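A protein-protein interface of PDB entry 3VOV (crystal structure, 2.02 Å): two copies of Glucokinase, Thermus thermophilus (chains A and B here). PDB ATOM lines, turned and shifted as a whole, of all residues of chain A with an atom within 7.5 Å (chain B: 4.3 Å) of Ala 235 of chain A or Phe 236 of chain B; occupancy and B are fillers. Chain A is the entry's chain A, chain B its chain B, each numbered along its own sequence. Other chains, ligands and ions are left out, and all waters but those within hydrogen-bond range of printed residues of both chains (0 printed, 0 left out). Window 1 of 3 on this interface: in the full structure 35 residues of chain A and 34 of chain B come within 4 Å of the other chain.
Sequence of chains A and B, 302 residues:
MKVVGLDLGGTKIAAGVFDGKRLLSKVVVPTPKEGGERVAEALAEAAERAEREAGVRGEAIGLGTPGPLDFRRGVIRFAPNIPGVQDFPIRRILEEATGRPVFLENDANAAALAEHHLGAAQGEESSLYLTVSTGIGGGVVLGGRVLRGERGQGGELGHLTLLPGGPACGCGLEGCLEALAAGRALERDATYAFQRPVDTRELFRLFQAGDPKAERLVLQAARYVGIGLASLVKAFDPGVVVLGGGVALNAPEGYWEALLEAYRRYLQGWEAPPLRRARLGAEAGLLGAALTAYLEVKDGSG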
ATOM      1  N   LEU A 128      21.414 -21.914  -6.327  1.00  0.00           N
ATOM      2  CA  LEU A 128      20.967 -21.166  -5.182  1.00  0.00           C
ATOM      3  C   LEU A 128      19.491 -21.467  -5.028  1.00  0.00           C
ATOM      4  O   LEU A 128      18.750 -21.419  -5.996  1.00  0.00           O
ATOM      5  CB  LEU A 128      21.228 -19.685  -5.434  1.00  0.00           C
ATOM      6  CG  LEU A 128      20.927 -18.781  -4.278  1.00  0.00           C
ATOM      7  CD1 LEU A 128      22.028 -17.724  -4.183  1.00  0.00           C
ATOM      8  CD2 LEU A 128      19.543 -18.166  -4.529  1.00  0.00           C
ATOM      9  N   VAL A 140      22.760 -22.369  -0.498  1.00  0.00           N
ATOM     10  CA  VAL A 140      23.667 -22.190  -1.615  1.00  0.00           C
ATOM     11  C   VAL A 140      24.487 -23.467  -1.726  1.00  0.00           C
ATOM     12  O   VAL A 140      25.105 -23.916  -0.741  1.00  0.00           O
ATOM     13  CB  VAL A 140      24.598 -20.997  -1.336  1.00  0.00           C
ATOM     14  CG1 VAL A 140      25.638 -20.791  -2.478  1.00  0.00           C
ATOM     15  CG2 VAL A 140      23.763 -19.736  -1.185  1.00  0.00           C
ATOM     16  N   LEU A 142      27.570 -25.038  -3.764  1.00  0.00           N
ATOM     17  CA  LEU A 142      28.723 -24.749  -4.550  1.00  0.00           C
ATOM     18  C   LEU A 142      29.697 -25.895  -4.672  1.00  0.00           C
ATOM     19  O   LEU A 142      29.961 -26.615  -3.736  1.00  0.00           O
ATOM     20  CB  LEU A 142      29.539 -23.619  -3.856  1.00  0.00           C
ATOM     21  CG  LEU A 142      28.867 -22.265  -3.518  1.00  0.00           C
ATOM     22  CD1 LEU A 142      29.789 -21.323  -2.728  1.00  0.00           C
ATOM     23  CD2 LEU A 142      28.396 -21.563  -4.788  1.00  0.00           C
ATOM     24  N   LEU A 147      27.109 -24.465   1.210  1.00  0.00           N
ATOM     25  CA  LEU A 147      27.937 -23.422   1.840  1.00  0.00           C
ATOM     26  C   LEU A 147      27.384 -23.217   3.263  1.00  0.00           C
ATOM     27  O   LEU A 147      26.292 -22.707   3.396  1.00  0.00           O
ATOM     28  CB  LEU A 147      27.745 -22.099   1.107  1.00  0.00           C
ATOM     29  CG  LEU A 147      28.834 -20.977   1.116  1.00  0.00           C
ATOM     30  CD1 LEU A 147      28.204 -19.605   1.229  1.00  0.00           C
ATOM     31  CD2 LEU A 147      29.941 -21.165   2.122  1.00  0.00           C
ATOM     32  N   ARG A 148      28.120 -23.616   4.290  1.00  0.00           N
ATOM     33  CA  ARG A 148      27.598 -23.587   5.672  1.00  0.00           C
ATOM     34  C   ARG A 148      28.012 -22.352   6.448  1.00  0.00           C
ATOM     35  O   ARG A 148      27.325 -21.941   7.394  1.00  0.00           O
ATOM     36  CB  ARG A 148      28.045 -24.836   6.445  1.00  0.00           C
ATOM     37  CG  ARG A 148      27.490 -26.120   5.858  1.00  0.00           C
ATOM     38  CD  ARG A 148      27.519 -27.269   6.850  1.00  0.00           C
ATOM     39  NE  ARG A 148      27.013 -28.514   6.263  1.00  0.00           N
ATOM     40  CZ  ARG A 148      27.708 -29.656   6.202  1.00  0.00           C
ATOM     41  NH1 ARG A 148      28.950 -29.727   6.676  1.00  0.00           N
ATOM     42  NH2 ARG A 148      27.170 -30.740   5.642  1.00  0.00           N
ATOM     43  N   GLY A 149      29.141 -21.768   6.059  1.00  0.00           N
ATOM     44  CA  GLY A 149      29.679 -20.589   6.735  1.00  0.00           C
ATOM     45  C   GLY A 149      30.614 -20.952   7.872  1.00  0.00           C
ATOM     46  O   GLY A 149      30.579 -22.082   8.383  1.00  0.00           O
ATOM     47  N   GLU A 150      31.430 -20.003   8.301  1.00  0.00           N
ATOM     48  CA  GLU A 150      32.361 -20.269   9.400  1.00  0.00           C
ATOM     49  C   GLU A 150      31.608 -20.612  10.718  1.00  0.00           C
ATOM     50  O   GLU A 150      32.079 -21.382  11.551  1.00  0.00           O
ATOM     51  CB  GLU A 150      33.300 -19.059   9.535  1.00  0.00           C
ATOM     52  CG  GLU A 150      34.130 -18.936  10.795  1.00  0.00           C
ATOM     53  CD  GLU A 150      35.403 -19.771  10.776  1.00  0.00           C
ATOM     54  OE1 GLU A 150      35.831 -20.223   9.679  1.00  0.00           O
ATOM     55  OE2 GLU A 150      35.969 -19.961  11.879  1.00  0.00           O
ATOM     56  N   ARG A 151      30.411 -20.065  10.851  1.00  0.00           N
ATOM     57  CA  ARG A 151      29.631 -20.167  12.082  1.00  0.00           C
ATOM     58  C   ARG A 151      28.287 -20.881  11.896  1.00  0.00           C
ATOM     59  O   ARG A 151      27.421 -20.791  12.753  1.00  0.00           O
ATOM     60  CB  ARG A 151      29.405 -18.762  12.635  1.00  0.00           C
ATOM     61  CG  ARG A 151      30.712 -18.074  13.080  1.00  0.00           C
ATOM     62  CD  ARG A 151      30.432 -16.600  13.389  1.00  0.00           C
ATOM     63  NE  ARG A 151      31.654 -15.813  13.266  1.00  0.00           N
ATOM     64  CZ  ARG A 151      32.193 -15.472  12.097  1.00  0.00           C
ATOM     65  NH1 ARG A 151      31.604 -15.818  10.934  1.00  0.00           N
ATOM     66  NH2 ARG A 151      33.326 -14.806  12.099  1.00  0.00           N
ATOM     67  N   GLN A 153      26.071 -19.864   9.828  1.00  0.00           N
ATOM     68  CA  GLN A 153      25.093 -18.852   9.399  1.00  0.00           C
ATOM     69  C   GLN A 153      25.052 -18.663   7.869  1.00  0.00           C
ATOM     70  O   GLN A 153      24.327 -17.786   7.377  1.00  0.00           O
ATOM     71  CB  GLN A 153      25.370 -17.449  10.014  1.00  0.00           C
ATOM     72  CG  GLN A 153      25.461 -17.344  11.512  1.00  0.00           C
ATOM     73  CD  GLN A 153      25.815 -15.915  11.983  1.00  0.00           C
ATOM     74  OE1 GLN A 153      25.130 -15.353  12.867  1.00  0.00           O
ATOM     75  NE2 GLN A 153      26.897 -15.316  11.392  1.00  0.00           N
ATOM     76  N   GLY A 154      25.822 -19.436   7.104  1.00  0.00           N
ATOM     77  CA  GLY A 154      25.824 -19.248   5.632  1.00  0.00           C
ATOM     78  C   GLY A 154      24.484 -19.592   5.026  1.00  0.00           C
ATOM     79  O   GLY A 154      23.765 -20.449   5.553  1.00  0.00           O
ATOM     80  N   GLY A 155      24.129 -18.941   3.927  1.00  0.00           N
ATOM     81  CA  GLY A 155      22.894 -19.261   3.280  1.00  0.00           C
ATOM     82  C   GLY A 155      21.647 -18.763   4.009  1.00  0.00           C
ATOM     83  O   GLY A 155      20.579 -19.269   3.742  1.00  0.00           O
ATOM     84  N   GLU A 156      21.772 -17.726   4.849  1.00  0.00           N
ATOM     85  CA  GLU A 156      20.604 -17.162   5.571  1.00  0.00           C
ATOM     86  C   GLU A 156      19.947 -16.140   4.673  1.00  0.00           C
ATOM     87  O   GLU A 156      19.894 -14.946   4.977  1.00  0.00           O
ATOM     88  CB  GLU A 156      21.023 -16.563   6.935  1.00  0.00           C
ATOM     89  CG  GLU A 156      21.128 -17.648   8.027  1.00  0.00           C
ATOM     90  CD  GLU A 156      19.759 -18.225   8.460  1.00  0.00           C
ATOM     91  OE1 GLU A 156      18.676 -17.692   8.130  1.00  0.00           O
ATOM     92  OE2 GLU A 156      19.757 -19.237   9.162  1.00  0.00           O
ATOM     93  N   LEU A 157      19.527 -16.632   3.519  1.00  0.00           N
ATOM     94  CA  LEU A 157      19.100 -15.812   2.389  1.00  0.00           C
ATOM     95  C   LEU A 157      17.867 -14.933   2.671  1.00  0.00           C
ATOM     96  O   LEU A 157      17.668 -13.946   1.990  1.00  0.00           O
ATOM     97  CB  LEU A 157      18.880 -16.698   1.133  1.00  0.00           C
ATOM     98  CG  LEU A 157      20.051 -17.606   0.652  1.00  0.00           C
ATOM     99  CD1 LEU A 157      19.749 -18.237  -0.703  1.00  0.00           C
ATOM    100  CD2 LEU A 157      21.402 -16.838   0.535  1.00  0.00           C
ATOM    101  N   LEU A 160      18.934 -11.104   4.035  1.00  0.00           N
ATOM    102  CA  LEU A 160      19.566  -9.971   3.322  1.00  0.00           C
ATOM    103  C   LEU A 160      18.650  -8.756   3.414  1.00  0.00           C
ATOM    104  O   LEU A 160      17.442  -8.873   3.265  1.00  0.00           O
ATOM    105  CB  LEU A 160      19.871 -10.327   1.863  1.00  0.00           C
ATOM    106  CG  LEU A 160      21.289 -11.006   1.917  1.00  0.00           C
ATOM    107  CD1 LEU A 160      21.153 -12.546   1.995  1.00  0.00           C
ATOM    108  CD2 LEU A 160      22.242 -10.617   0.784  1.00  0.00           C
ATOM    109  N   LEU A 229      16.564 -12.234  -5.227  1.00  0.00           N
ATOM    110  CA  LEU A 229      17.236 -13.289  -6.019  1.00  0.00           C
ATOM    111  C   LEU A 229      18.224 -12.704  -7.010  1.00  0.00           C
ATOM    112  O   LEU A 229      19.325 -13.225  -7.157  1.00  0.00           O
ATOM    113  CB  LEU A 229      16.211 -14.154  -6.752  1.00  0.00           C
ATOM    114  CG  LEU A 229      15.404 -15.006  -5.758  1.00  0.00           C
ATOM    115  CD1 LEU A 229      14.189 -15.685  -6.428  1.00  0.00           C
ATOM    116  CD2 LEU A 229      16.323 -16.048  -5.079  1.00  0.00           C
ATOM    117  N   ALA A 230      17.863 -11.596  -7.651  1.00  0.00           N
ATOM    118  CA  ALA A 230      18.771 -10.966  -8.645  1.00  0.00           C
ATOM    119  C   ALA A 230      20.009 -10.424  -7.973  1.00  0.00           C
ATOM    120  O   ALA A 230      21.123 -10.491  -8.506  1.00  0.00           O
ATOM    121  CB  ALA A 230      18.060  -9.857  -9.387  1.00  0.00           C
ATOM    122  N   SER A 231      19.816  -9.881  -6.782  1.00  0.00           N
ATOM    123  CA  SER A 231      20.904  -9.365  -5.980  1.00  0.00           C
ATOM    124  C   SER A 231      21.903 -10.476  -5.574  1.00  0.00           C
ATOM    125  O   SER A 231      23.146 -10.313  -5.677  1.00  0.00           O
ATOM    126  CB  SER A 231      20.274  -8.728  -4.745  1.00  0.00           C
ATOM    127  OG  SER A 231      21.006  -7.635  -4.411  1.00  0.00           O
ATOM    128  N   LEU A 232      21.349 -11.607  -5.127  1.00  0.00           N
ATOM    129  CA  LEU A 232      22.128 -12.805  -4.777  1.00  0.00           C
ATOM    130  C   LEU A 232      22.912 -13.382  -5.966  1.00  0.00           C
ATOM    131  O   LEU A 232      23.989 -13.983  -5.801  1.00  0.00           O
ATOM    132  CB  LEU A 232      21.199 -13.860  -4.210  1.00  0.00           C
ATOM    133  CG  LEU A 232      20.740 -13.557  -2.768  1.00  0.00           C
ATOM    134  CD1 LEU A 232      19.535 -14.430  -2.303  1.00  0.00           C
ATOM    135  CD2 LEU A 232      21.917 -13.744  -1.818  1.00  0.00           C
ATOM    136  N   VAL A 233      22.394 -13.179  -7.181  1.00  0.00           N
ATOM    137  CA  VAL A 233      23.138 -13.584  -8.395  1.00  0.00           C
ATOM    138  C   VAL A 233      24.463 -12.822  -8.458  1.00  0.00           C
ATOM    139  O   VAL A 233      25.508 -13.397  -8.842  1.00  0.00           O
ATOM    140  CB  VAL A 233      22.307 -13.346  -9.695  1.00  0.00           C
ATOM    141  CG1 VAL A 233      23.197 -13.559 -10.960  1.00  0.00           C
ATOM    142  CG2 VAL A 233      21.181 -14.277  -9.726  1.00  0.00           C
ATOM    143  N   LYS A 234      24.464 -11.545  -8.063  1.00  0.00           N
ATOM    144  CA  LYS A 234      25.748 -10.782  -8.122  1.00  0.00           C
ATOM    145  C   LYS A 234      26.707 -11.307  -7.091  1.00  0.00           C
ATOM    146  O   LYS A 234      27.900 -11.201  -7.263  1.00  0.00           O
ATOM    147  CB  LYS A 234      25.577  -9.284  -7.885  1.00  0.00           C
ATOM    148  CG  LYS A 234      24.294  -8.649  -8.399  1.00  0.00           C
ATOM    149  CD  LYS A 234      24.088  -8.865  -9.825  1.00  0.00           C
ATOM    150  CE  LYS A 234      23.045  -7.814 -10.335  1.00  0.00           C
ATOM    151  NZ  LYS A 234      21.637  -8.024  -9.800  1.00  0.00           N
ATOM    152  N   ALA A 235      26.188 -11.859  -5.995  1.00  0.00           N
ATOM    153  CA  ALA A 235      27.095 -12.381  -4.950  1.00  0.00           C
ATOM    154  C   ALA A 235      27.669 -13.720  -5.391  1.00  0.00           C
ATOM    155  O   ALA A 235      28.891 -13.907  -5.360  1.00  0.00           O
ATOM    156  CB  ALA A 235      26.371 -12.518  -3.620  1.00  0.00           C
ATOM    157  N   PHE A 236      26.784 -14.612  -5.846  1.00  0.00           N
ATOM    158  CA  PHE A 236      27.099 -16.005  -5.985  1.00  0.00           C
ATOM    159  C   PHE A 236      27.246 -16.508  -7.437  1.00  0.00           C
ATOM    160  O   PHE A 236      27.878 -17.538  -7.630  1.00  0.00           O
ATOM    161  CB  PHE A 236      26.028 -16.865  -5.300  1.00  0.00           C
ATOM    162  CG  PHE A 236      26.082 -16.853  -3.789  1.00  0.00           C
ATOM    163  CD1 PHE A 236      27.053 -17.567  -3.099  1.00  0.00           C
ATOM    164  CD2 PHE A 236      25.133 -16.144  -3.065  1.00  0.00           C
ATOM    165  CE1 PHE A 236      27.108 -17.531  -1.701  1.00  0.00           C
ATOM    166  CE2 PHE A 236      25.150 -16.124  -1.692  1.00  0.00           C
ATOM    167  CZ  PHE A 236      26.139 -16.813  -0.989  1.00  0.00           C
ATOM    168  N   ASP A 237      26.600 -15.846  -8.408  1.00  0.00           N
ATOM    169  CA  ASP A 237      26.592 -16.278  -9.823  1.00  0.00           C
ATOM    170  C   ASP A 237      26.362 -17.814 -10.009  1.00  0.00           C
ATOM    171  O   ASP A 237      27.214 -18.517 -10.588  1.00  0.00           O
ATOM    172  CB  ASP A 237      27.875 -15.810 -10.518  1.00  0.00           C
ATOM    173  CG  ASP A 237      27.869 -16.059 -12.049  1.00  0.00           C
ATOM    174  OD1 ASP A 237      26.788 -16.015 -12.690  1.00  0.00           O
ATOM    175  OD2 ASP A 237      28.978 -16.236 -12.603  1.00  0.00           O
ATOM    176  N   PRO A 238      25.206 -18.320  -9.506  1.00  0.00           N
ATOM    177  CA  PRO A 238      24.861 -19.736  -9.498  1.00  0.00           C
ATOM    178  C   PRO A 238      24.474 -20.176 -10.903  1.00  0.00           C
ATOM    179  O   PRO A 238      24.036 -19.352 -11.707  1.00  0.00           O
ATOM    180  CB  PRO A 238      23.655 -19.780  -8.568  1.00  0.00           C
ATOM    181  CG  PRO A 238      22.983 -18.413  -8.784  1.00  0.00           C
ATOM    182  CD  PRO A 238      24.121 -17.480  -8.910  1.00  0.00           C
ATOM    183  N   TRP A 270      23.326  -7.744 -16.956  1.00  0.00           N
ATOM    184  CA  TRP A 270      23.952  -8.943 -16.374  1.00  0.00           C
ATOM    185  C   TRP A 270      23.504 -10.158 -17.144  1.00  0.00           C
ATOM    186  O   TRP A 270      22.504 -10.096 -17.823  1.00  0.00           O
ATOM    187  CB  TRP A 270      23.545  -9.104 -14.865  1.00  0.00           C
ATOM    188  CG  TRP A 270      24.068  -7.933 -14.035  1.00  0.00           C
ATOM    189  CD1 TRP A 270      23.503  -6.694 -13.913  1.00  0.00           C
ATOM    190  CD2 TRP A 270      25.284  -7.899 -13.283  1.00  0.00           C
ATOM    191  NE1 TRP A 270      24.289  -5.887 -13.142  1.00  0.00           N
ATOM    192  CE2 TRP A 270      25.394  -6.596 -12.737  1.00  0.00           C
ATOM    193  CE3 TRP A 270      26.287  -8.852 -13.009  1.00  0.00           C
ATOM    194  CZ2 TRP A 270      26.462  -6.208 -11.929  1.00  0.00           C
ATOM    195  CZ3 TRP A 270      27.380  -8.470 -12.229  1.00  0.00           C
ATOM    196  CH2 TRP A 270      27.447  -7.152 -11.671  1.00  0.00           C
ATOM    197  N   LEU B 128      35.703 -12.246   3.184  1.00  0.00           N
ATOM    198  CA  LEU B 128      34.933 -11.453   2.270  1.00  0.00           C
ATOM    199  C   LEU B 128      35.639 -10.118   2.227  1.00  0.00           C
ATOM    200  O   LEU B 128      35.960  -9.552   3.264  1.00  0.00           O
ATOM    201  CB  LEU B 128      33.550 -11.333   2.887  1.00  0.00           C
ATOM    202  CG  LEU B 128      32.365 -10.556   2.390  1.00  0.00           C
ATOM    203  CD1 LEU B 128      32.776  -9.199   1.951  1.00  0.00           C
ATOM    204  CD2 LEU B 128      31.538 -11.330   1.360  1.00  0.00           C
ATOM    205  N   VAL B 140      35.094 -12.865  -2.862  1.00  0.00           N
ATOM    206  CA  VAL B 140      34.763 -13.860  -1.874  1.00  0.00           C
ATOM    207  C   VAL B 140      35.749 -15.028  -1.971  1.00  0.00           C
ATOM    208  O   VAL B 140      35.950 -15.595  -3.057  1.00  0.00           O
ATOM    209  CB  VAL B 140      33.331 -14.394  -2.073  1.00  0.00           C
ATOM    210  CG1 VAL B 140      32.957 -15.262  -0.855  1.00  0.00           C
ATOM    211  CG2 VAL B 140      32.339 -13.213  -2.175  1.00  0.00           C
ATOM    212  N   LEU B 147      35.822 -17.349  -5.165  1.00  0.00           N
ATOM    213  CA  LEU B 147      34.528 -17.733  -5.747  1.00  0.00           C
ATOM    214  C   LEU B 147      34.367 -16.999  -7.072  1.00  0.00           C
ATOM    215  O   LEU B 147      34.159 -15.811  -7.089  1.00  0.00           O
ATOM    216  CB  LEU B 147      33.382 -17.285  -4.819  1.00  0.00           C
ATOM    217  CG  LEU B 147      32.057 -18.040  -4.663  1.00  0.00           C
ATOM    218  CD1 LEU B 147      30.860 -17.057  -4.375  1.00  0.00           C
ATOM    219  CD2 LEU B 147      31.728 -19.058  -5.739  1.00  0.00           C
ATOM    220  N   GLY B 154      30.675 -14.013 -10.134  1.00  0.00           N
ATOM    221  CA  GLY B 154      30.683 -14.190  -8.691  1.00  0.00           C
ATOM    222  C   GLY B 154      31.458 -13.089  -8.005  1.00  0.00           C
ATOM    223  O   GLY B 154      32.449 -12.548  -8.574  1.00  0.00           O
ATOM    224  N   GLY B 155      31.000 -12.708  -6.808  1.00  0.00           N
ATOM    225  CA  GLY B 155      31.742 -11.715  -6.002  1.00  0.00           C
ATOM    226  C   GLY B 155      31.700 -10.304  -6.559  1.00  0.00           C
ATOM    227  O   GLY B 155      32.598  -9.531  -6.309  1.00  0.00           O
ATOM    228  N   LEU B 232      25.827  -9.098   3.356  1.00  0.00           N
ATOM    229  CA  LEU B 232      26.727 -10.135   2.793  1.00  0.00           C
ATOM    230  C   LEU B 232      27.133 -11.189   3.815  1.00  0.00           C
ATOM    231  O   LEU B 232      27.342 -12.337   3.474  1.00  0.00           O
ATOM    232  CB  LEU B 232      27.978  -9.479   2.149  1.00  0.00           C
ATOM    233  CG  LEU B 232      27.628  -8.772   0.816  1.00  0.00           C
ATOM    234  CD1 LEU B 232      28.711  -7.774   0.347  1.00  0.00           C
ATOM    235  CD2 LEU B 232      27.328  -9.838  -0.292  1.00  0.00           C
ATOM    236  N   VAL B 233      27.230 -10.812   5.083  1.00  0.00           N
ATOM    237  CA  VAL B 233      27.503 -11.798   6.139  1.00  0.00           C
ATOM    238  C   VAL B 233      26.385 -12.848   6.226  1.00  0.00           C
ATOM    239  O   VAL B 233      26.643 -14.021   6.491  1.00  0.00           O
ATOM    240  CB  VAL B 233      27.714 -11.102   7.495  1.00  0.00           C
ATOM    241  CG1 VAL B 233      27.654 -12.139   8.684  1.00  0.00           C
ATOM    242  CG2 VAL B 233      29.050 -10.355   7.471  1.00  0.00           C
ATOM    243  N   LYS B 234      25.146 -12.443   5.958  1.00  0.00           N
ATOM    244  CA  LYS B 234      24.035 -13.403   6.030  1.00  0.00           C
ATOM    245  C   LYS B 234      24.155 -14.421   4.883  1.00  0.00           C
ATOM    246  O   LYS B 234      23.736 -15.573   4.990  1.00  0.00           O
ATOM    247  CB  LYS B 234      22.669 -12.684   5.888  1.00  0.00           C
ATOM    248  CG  LYS B 234      22.477 -11.415   6.743  1.00  0.00           C
ATOM    249  CD  LYS B 234      22.575 -11.693   8.204  1.00  0.00           C
ATOM    250  CE  LYS B 234      22.104 -10.456   8.996  1.00  0.00           C
ATOM    251  NZ  LYS B 234      22.703  -9.138   8.552  1.00  0.00           N
ATOM    252  N   ALA B 235      24.668 -13.976   3.745  1.00  0.00           N
ATOM    253  CA  ALA B 235      24.759 -14.885   2.637  1.00  0.00           C
ATOM    254  C   ALA B 235      25.987 -15.800   2.828  1.00  0.00           C
ATOM    255  O   ALA B 235      25.880 -17.011   2.624  1.00  0.00           O
ATOM    256  CB  ALA B 235      24.848 -14.108   1.344  1.00  0.00           C
ATOM    257  N   PHE B 236      27.132 -15.230   3.245  1.00  0.00           N
ATOM    258  CA  PHE B 236      28.389 -15.966   3.227  1.00  0.00           C
ATOM    259  C   PHE B 236      28.911 -16.454   4.575  1.00  0.00           C
ATOM    260  O   PHE B 236      29.625 -17.458   4.592  1.00  0.00           O
ATOM    261  CB  PHE B 236      29.493 -15.130   2.545  1.00  0.00           C
ATOM    262  CG  PHE B 236      29.275 -14.903   1.090  1.00  0.00           C
ATOM    263  CD1 PHE B 236      29.610 -15.888   0.156  1.00  0.00           C
ATOM    264  CD2 PHE B 236      28.758 -13.682   0.627  1.00  0.00           C
ATOM    265  CE1 PHE B 236      29.430 -15.669  -1.215  1.00  0.00           C
ATOM    266  CE2 PHE B 236      28.568 -13.463  -0.746  1.00  0.00           C
ATOM    267  CZ  PHE B 236      28.893 -14.457  -1.665  1.00  0.00           C
ATOM    268  N   ASP B 237      28.609 -15.734   5.676  1.00  0.00           N
ATOM    269  CA  ASP B 237      29.087 -16.071   7.036  1.00  0.00           C
ATOM    270  C   ASP B 237      30.610 -16.289   7.000  1.00  0.00           C
ATOM    271  O   ASP B 237      31.095 -17.372   7.353  1.00  0.00           O
ATOM    272  CB  ASP B 237      28.352 -17.312   7.607  1.00  0.00           C
ATOM    273  CG  ASP B 237      28.719 -17.613   9.080  1.00  0.00           C
ATOM    274  OD1 ASP B 237      29.200 -16.709   9.804  1.00  0.00           O
ATOM    275  OD2 ASP B 237      28.495 -18.764   9.509  1.00  0.00           O
ATOM    276  N   PRO B 238      31.366 -15.265   6.544  1.00  0.00           N
ATOM    277  CA  PRO B 238      32.800 -15.422   6.338  1.00  0.00           C
ATOM    278  C   PRO B 238      33.543 -15.361   7.671  1.00  0.00           C
ATOM    279  O   PRO B 238      33.025 -14.798   8.633  1.00  0.00           O
ATOM    280  CB  PRO B 238      33.144 -14.185   5.502  1.00  0.00           C
ATOM    281  CG  PRO B 238      32.179 -13.129   6.022  1.00  0.00           C
ATOM    282  CD  PRO B 238      30.901 -13.898   6.211  1.00  0.00           C
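The backbone NH (N) of Gln 153 of chain A sits at hydrogen-bond distance from the backbone carbonyl oxygen (O) of Arg 148 of chain A, 3.4 Å away. The backbone NH (N) of Leu 147 of chain A lies within hydrogen-bond range of the backbone carbonyl oxygen (O) of Val 140 of chain A, at 2.9 Å. The backbone carbonyl oxygen (O) of Val 140 of chain B sits at hydrogen-bond distance from the backbone NH (N) of Leu 147 of chain B. The backbone carbonyl oxygen of Arg 148 of chain A is in hydrogen-bond range of the backbone NH of Gly 154 of chain A, at 2.9 Å. NZ of Lys 234 of chain A lies within hydrogen-bond range of O of Ala 230 of chain A (2.8 Å).
The guanidinium group (NH1) of Arg 151 of chain A sits at hydrogen-bond distance from the backbone carbonyl oxygen (O) of Pro 238 of chain B, at 2.9 Å. The side-chain carboxylate (OD1) of Asp 237 of chain B is in salt-bridge range of the guanidinium group (NH1) of Arg 151 of chain A (2.8 Å). The backbone carbonyl oxygen (O) of Gln 153 of chain A sits close to the backbone carbonyl oxygen (O) of Lys 234 of chain B (3.3 Å). The backbone NH of Glu 156 of chain A sits at hydrogen-bond distance from the backbone carbonyl oxygen of Lys 234 of chain B. The backbone NH of Gln 153 of chain A lies within hydrogen-bond range of the side-chain carboxylate of Asp 237 of chain B (2.7 Å). The backbone carbonyl oxygen (O) of Lys 234 of chain A sits at hydrogen-bond distance from the backbone NH (N) of Gly 155 of chain B, 3.5 Å away. The backbone NH of Glu 150 of chain A is in hydrogen-bond range of the backbone carbonyl oxygen of Asp 237 of chain B (2.8 Å). The backbone NH (N) of Gly 155 of chain A sits at hydrogen-bond distance from the backbone carbonyl oxygen (O) of Ala 235 of chain B. O of Ala 235 of chain A sits at hydrogen-bond distance from N of Gly 155 of chain B, 2.8 Å away.
Ala 235 of chain A touches just these residues of chain B: Leu 147, Gly 154, Gly 155 and Phe 236. Of chain A, only Gly 149 (3.8 Å), Ala 235 (3.7 Å) and Phe 236 (3.0 Å) come within 4 Å of Phe 236 of chain B. Of the printed residues of chain B, Arg 148 of chain A touches Asp 237 (3.99 Å). Of the printed residues of chain B, Leu 147 of chain A touches Ala 235 (3.8 Å). Printed residues of chain B within 4 Å of Glu 156 of chain A: Lys 234 (2.9 Å). Leu 157 of chain A touches none of the printed residues of chain B. Leu 160 of chain A touches none of the printed residues of chain B. The nearest residue of chain A that does not touch Phe 236 of chain B is Leu 147 of chain A (4.1 Å).
Ala 235 of chain B touches Leu 147 of chain A. Asp 237 of chain B touches Arg 148 of chain A (OD2 to O, 3.99 Å). Phe 236 of chain B touches Gly 149 of chain A (O to CA, 3.8 Å). Gly 149 of chain A touches Asp 237 of chain B. N of Gly 154 of chain A touches CB of Asp 237 of chain B, at 3.3 Å. Gly 155 of chain A touches Lys 234 of chain B. Ala 235 of chain A touches Leu 147 of chain B (O to CD1, 3.8 Å). Ala 235 of chain A touches Gly 154 of chain B (O to C, 3.8 Å). Phe 236 of chain A touches Phe 236 of chain B. N of Gly 154 of chain B touches CB of Asp 237 of chain A (3.3 Å).
Printed residues of chain B that touch a printed residue of chain A: Leu 147, Gly 154, Gly 155, Lys 234, Ala 235, Phe 236, Asp 237 and Pro 238. Hydrophobic or aromatic side chains of chain B that line the printed part of chain A: Leu 147, Ala 235 and Phe 236. Hydrophobic or aromatic side chains of chain A within 4 Å of the printed part of chain B: Leu 147, Ala 235 and Phe 236. Among the printed residues, 22 pairs touch across the chains.
Gly 154 of chain A touches Asp 237 of chain B, and with the chains exchanged Asp 237 of chain A touches Gly 154 of chain B. Gly 155 of chain A touches Lys 234 of chain B, and with the chains exchanged Lys 234 of chain A touches Gly 155 of chain B. Ala 235 of chain A touches Phe 236 of chain B, and with the chains exchanged Phe 236 of chain A touches Ala 235 of chain B. Phe 236 of chain B touches its own counterpart, Phe 236 of chain A. Positions printed for both chains: 128, 140, 147, 154, 155, 232, 233, 234, 235, 236, 237 and 238. Of the 22 pairs that touch across the chains among the printed residues, 13 have their exchanged pair printed and touching as well.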
